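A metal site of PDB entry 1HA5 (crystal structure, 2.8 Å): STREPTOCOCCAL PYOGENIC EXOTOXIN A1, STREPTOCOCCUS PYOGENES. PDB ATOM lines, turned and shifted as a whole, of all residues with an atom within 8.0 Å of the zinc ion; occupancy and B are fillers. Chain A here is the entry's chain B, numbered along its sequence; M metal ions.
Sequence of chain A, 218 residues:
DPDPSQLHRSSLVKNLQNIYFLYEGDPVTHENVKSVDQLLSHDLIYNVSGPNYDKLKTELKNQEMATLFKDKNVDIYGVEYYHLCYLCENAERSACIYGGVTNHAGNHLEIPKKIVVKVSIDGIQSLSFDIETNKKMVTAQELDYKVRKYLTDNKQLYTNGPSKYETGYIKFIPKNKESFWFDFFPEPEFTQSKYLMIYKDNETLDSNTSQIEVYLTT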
ATOM      1  N   HIS A  30      20.204   7.809 -30.167  1.00  0.00           N
ATOM      2  CA  HIS A  30      19.266   8.047 -29.085  1.00  0.00           C
ATOM      3  C   HIS A  30      18.894   9.516 -29.153  1.00  0.00           C
ATOM      4  O   HIS A  30      19.731  10.355 -29.494  1.00  0.00           O
ATOM      5  CB  HIS A  30      19.899   7.654 -27.754  1.00  0.00           C
ATOM      6  CG  HIS A  30      20.247   6.203 -27.687  1.00  0.00           C
ATOM      7  ND1 HIS A  30      21.444   5.700 -28.170  1.00  0.00           N
ATOM      8  CD2 HIS A  30      19.521   5.130 -27.325  1.00  0.00           C
ATOM      9  CE1 HIS A  30      21.425   4.384 -28.098  1.00  0.00           C
ATOM     10  NE2 HIS A  30      20.265   4.007 -27.589  1.00  0.00           N
ATOM     11  N   GLU A  31      17.644   9.827 -28.853  1.00  0.00           N
ATOM     12  CA  GLU A  31      17.163  11.195 -28.967  1.00  0.00           C
ATOM     13  C   GLU A  31      17.249  12.154 -27.799  1.00  0.00           C
ATOM     14  O   GLU A  31      18.192  12.935 -27.694  1.00  0.00           O
ATOM     15  CB  GLU A  31      15.729  11.196 -29.480  1.00  0.00           C
ATOM     16  CG  GLU A  31      15.648  11.152 -30.989  1.00  0.00           C
ATOM     17  CD  GLU A  31      16.538  12.213 -31.631  1.00  0.00           C
ATOM     18  OE1 GLU A  31      16.442  13.377 -31.187  1.00  0.00           O
ATOM     19  OE2 GLU A  31      17.319  11.888 -32.557  1.00  0.00           O
ATOM     20  N   ASN A  32      16.247  12.112 -26.924  1.00  0.00           N
ATOM     21  CA  ASN A  32      16.213  13.033 -25.796  1.00  0.00           C
ATOM     22  C   ASN A  32      16.801  12.420 -24.524  1.00  0.00           C
ATOM     23  O   ASN A  32      16.063  12.144 -23.577  1.00  0.00           O
ATOM     24  CB  ASN A  32      14.766  13.459 -25.533  1.00  0.00           C
ATOM     25  CG  ASN A  32      14.669  14.772 -24.801  1.00  0.00           C
ATOM     26  OD1 ASN A  32      13.608  15.130 -24.282  1.00  0.00           O
ATOM     27  ND2 ASN A  32      15.761  15.517 -24.763  1.00  0.00           N
ATOM     28  N   VAL A  33      18.123  12.219 -24.489  1.00  0.00           N
ATOM     29  CA  VAL A  33      18.753  11.597 -23.323  1.00  0.00           C
ATOM     30  C   VAL A  33      19.707  12.457 -22.491  1.00  0.00           C
ATOM     31  O   VAL A  33      20.257  13.449 -22.955  1.00  0.00           O
ATOM     32  CB  VAL A  33      19.490  10.295 -23.699  1.00  0.00           C
ATOM     33  CG1 VAL A  33      18.503   9.309 -24.316  1.00  0.00           C
ATOM     34  CG2 VAL A  33      20.641  10.586 -24.655  1.00  0.00           C
ATOM     35  N   ASN A  73      20.070  17.412 -22.074  1.00  0.00           N
ATOM     36  CA  ASN A  73      19.319  16.495 -22.908  1.00  0.00           C
ATOM     37  C   ASN A  73      20.014  16.580 -24.260  1.00  0.00           C
ATOM     38  O   ASN A  73      19.995  17.621 -24.922  1.00  0.00           O
ATOM     39  CB  ASN A  73      17.856  16.933 -22.999  1.00  0.00           C
ATOM     40  CG  ASN A  73      17.121  16.771 -21.681  1.00  0.00           C
ATOM     41  OD1 ASN A  73      16.944  15.660 -21.188  1.00  0.00           O
ATOM     42  ND2 ASN A  73      16.700  17.889 -21.105  1.00  0.00           N
ATOM     43  N   VAL A  74      20.636  15.468 -24.661  1.00  0.00           N
ATOM     44  CA  VAL A  74      21.398  15.392 -25.906  1.00  0.00           C
ATOM     45  C   VAL A  74      20.954  14.297 -26.884  1.00  0.00           C
ATOM     46  O   VAL A  74      20.091  13.483 -26.567  1.00  0.00           O
ATOM     47  CB  VAL A  74      22.900  15.165 -25.600  1.00  0.00           C
ATOM     48  CG1 VAL A  74      23.446  16.346 -24.806  1.00  0.00           C
ATOM     49  CG2 VAL A  74      23.088  13.876 -24.812  1.00  0.00           C
ATOM     50  N   ASP A  75      21.566  14.299 -28.075  1.00  0.00           N
ATOM     51  CA  ASP A  75      21.304  13.293 -29.108  1.00  0.00           C
ATOM     52  C   ASP A  75      22.612  12.520 -29.306  1.00  0.00           C
ATOM     53  O   ASP A  75      23.696  13.099 -29.213  1.00  0.00           O
ATOM     54  CB  ASP A  75      20.918  13.935 -30.438  1.00  0.00           C
ATOM     55  CG  ASP A  75      19.471  14.397 -30.468  1.00  0.00           C
ATOM     56  OD1 ASP A  75      18.596  13.667 -29.954  1.00  0.00           O
ATOM     57  OD2 ASP A  75      19.209  15.483 -31.046  1.00  0.00           O
ATOM     58  N   ILE A  76      22.492  11.225 -29.567  1.00  0.00           N
ATOM     59  CA  ILE A  76      23.664  10.375 -29.775  1.00  0.00           C
ATOM     60  C   ILE A  76      23.577   9.752 -31.175  1.00  0.00           C
ATOM     61  O   ILE A  76      22.494   9.417 -31.664  1.00  0.00           O
ATOM     62  CB  ILE A  76      23.744   9.228 -28.733  1.00  0.00           C
ATOM     63  CG1 ILE A  76      23.898   9.796 -27.319  1.00  0.00           C
ATOM     64  CG2 ILE A  76      24.922   8.329 -29.025  1.00  0.00           C
ATOM     65  CD1 ILE A  76      23.921   8.733 -26.270  1.00  0.00           C
ATOM     66  N   THR A 102      25.359  15.716 -29.393  1.00  0.00           N
ATOM     67  CA  THR A 102      24.897  17.066 -29.690  1.00  0.00           C
ATOM     68  C   THR A 102      23.674  17.372 -28.842  1.00  0.00           C
ATOM     69  O   THR A 102      22.990  16.469 -28.371  1.00  0.00           O
ATOM     70  CB  THR A 102      24.507  17.221 -31.170  1.00  0.00           C
ATOM     71  OG1 THR A 102      23.366  16.406 -31.450  1.00  0.00           O
ATOM     72  CG2 THR A 102      25.654  16.812 -32.060  1.00  0.00           C
ATOM     73  N   ASN A 103      23.408  18.662 -28.645  1.00  0.00           N
ATOM     74  CA  ASN A 103      22.252  19.106 -27.885  1.00  0.00           C
ATOM     75  C   ASN A 103      20.973  18.779 -28.652  1.00  0.00           C
ATOM     76  O   ASN A 103      20.874  18.997 -29.874  1.00  0.00           O
ATOM     77  CB  ASN A 103      22.334  20.609 -27.627  1.00  0.00           C
ATOM     78  CG  ASN A 103      23.432  20.967 -26.654  1.00  0.00           C
ATOM     79  OD1 ASN A 103      23.572  20.335 -25.614  1.00  0.00           O
ATOM     80  ND2 ASN A 103      24.208  21.990 -26.986  1.00  0.00           N
ATOM     81  N   HIS A 104      19.987  18.269 -27.933  1.00  0.00           N
ATOM     82  CA  HIS A 104      18.716  17.907 -28.540  1.00  0.00           C
ATOM     83  C   HIS A 104      17.815  19.096 -28.846  1.00  0.00           C
ATOM     84  O   HIS A 104      17.224  19.159 -29.914  1.00  0.00           O
ATOM     85  CB  HIS A 104      17.982  16.911 -27.654  1.00  0.00           C
ATOM     86  CG  HIS A 104      16.506  16.870 -27.905  1.00  0.00           C
ATOM     87  ND1 HIS A 104      15.956  16.496 -29.117  1.00  0.00           N
ATOM     88  CD2 HIS A 104      15.459  17.193 -27.102  1.00  0.00           C
ATOM     89  CE1 HIS A 104      14.643  16.584 -29.050  1.00  0.00           C
ATOM     90  NE2 HIS A 104      14.311  17.013 -27.842  1.00  0.00           N
ATOM     91  N   ALA A 105      17.706  20.028 -27.890  1.00  0.00           N
ATOM     92  CA  ALA A 105      16.825  21.198 -28.046  1.00  0.00           C
ATOM     93  C   ALA A 105      17.316  22.268 -29.028  1.00  0.00           C
ATOM     94  O   ALA A 105      18.451  22.733 -28.943  1.00  0.00           O
ATOM     95  CB  ALA A 105      16.555  21.836 -26.652  1.00  0.00           C
ATOM     96  N   GLY A 106      16.437  22.633 -29.961  1.00  0.00           N
ATOM     97  CA  GLY A 106      16.756  23.636 -30.951  1.00  0.00           C
ATOM     98  C   GLY A 106      17.699  23.185 -32.057  1.00  0.00           C
ATOM     99  O   GLY A 106      18.220  24.002 -32.830  1.00  0.00           O
ATOM    100  N   ASN A 107      17.909  21.872 -32.156  1.00  0.00           N
ATOM    101  CA  ASN A 107      18.812  21.336 -33.153  1.00  0.00           C
ATOM    102  C   ASN A 107      18.114  20.527 -34.219  1.00  0.00           C
ATOM    103  O   ASN A 107      18.734  19.730 -34.922  1.00  0.00           O
ATOM    104  CB  ASN A 107      19.866  20.461 -32.492  1.00  0.00           C
ATOM    105  CG  ASN A 107      21.141  20.383 -33.300  1.00  0.00           C
ATOM    106  OD1 ASN A 107      21.826  19.365 -33.309  1.00  0.00           O
ATOM    107  ND2 ASN A 107      21.460  21.479 -33.990  1.00  0.00           N
ATOM    108  N   HIS A 108      16.813  20.732 -34.367  1.00  0.00           N
ATOM    109  CA  HIS A 108      16.097  19.977 -35.376  1.00  0.00           C
ATOM    110  C   HIS A 108      15.525  20.842 -36.500  1.00  0.00           C
ATOM    111  O   HIS A 108      15.246  22.038 -36.320  1.00  0.00           O
ATOM    112  CB  HIS A 108      14.968  19.176 -34.712  1.00  0.00           C
ATOM    113  CG  HIS A 108      15.440  17.997 -33.917  1.00  0.00           C
ATOM    114  ND1 HIS A 108      15.432  16.712 -34.414  1.00  0.00           N
ATOM    115  CD2 HIS A 108      15.930  17.906 -32.661  1.00  0.00           C
ATOM    116  CE1 HIS A 108      15.887  15.874 -33.501  1.00  0.00           C
ATOM    117  NE2 HIS A 108      16.195  16.572 -32.422  1.00  0.00           N
ATOM    118  N   ASN A 134      18.416  15.440 -39.669  1.00  0.00           N
ATOM    119  CA  ASN A 134      17.428  16.322 -39.078  1.00  0.00           C
ATOM    120  C   ASN A 134      18.148  17.149 -38.018  1.00  0.00           C
ATOM    121  O   ASN A 134      17.601  17.406 -36.947  1.00  0.00           O
ATOM    122  CB  ASN A 134      16.303  15.486 -38.468  1.00  0.00           C
ATOM    123  CG  ASN A 134      16.831  14.315 -37.651  1.00  0.00           C
ATOM    124  OD1 ASN A 134      17.750  13.623 -38.075  1.00  0.00           O
ATOM    125  ND2 ASN A 134      16.245  14.103 -36.476  1.00  0.00           N
ATOM    126  N   LYS A 135      19.375  17.549 -38.319  1.00  0.00           N
ATOM    127  CA  LYS A 135      20.168  18.336 -37.378  1.00  0.00           C
ATOM    128  C   LYS A 135      20.873  19.535 -37.983  1.00  0.00           C
ATOM    129  O   LYS A 135      21.580  19.414 -38.987  1.00  0.00           O
ATOM    130  CB  LYS A 135      21.223  17.468 -36.692  1.00  0.00           C
ATOM    131  CG  LYS A 135      20.713  16.737 -35.472  1.00  0.00           C
ATOM    132  CD  LYS A 135      21.849  16.123 -34.667  1.00  0.00           C
ATOM    133  CE  LYS A 135      22.281  14.778 -35.221  1.00  0.00           C
ATOM    134  NZ  LYS A 135      21.263  13.707 -34.999  1.00  0.00           N
HETATM  135 ZN    ZN M   1      16.872  15.235 -30.755  1.00  0.00          ZN
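A ring nitrogen (ND1) of His 108 lies close to the backbone carbonyl oxygen (O) of Asn 134 (3.4 Å).
O of Asn 73 sits at hydrogen-bond distance from N of His 104, 3.1 Å away.
The backbone NH (N) of Asp 75 lies within hydrogen-bond range of the backbone carbonyl oxygen (O) of Thr 102 (2.6 Å).
The zinc ion is bound by OE1 of Glu 31 (2.0 Å), NE2 of His 108 (2.2 Å), ND1 of His 104 (2.3 Å), OD2 of Asp 75 (2.4 Å) and OD1 of Asp 75 (2.5 Å).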
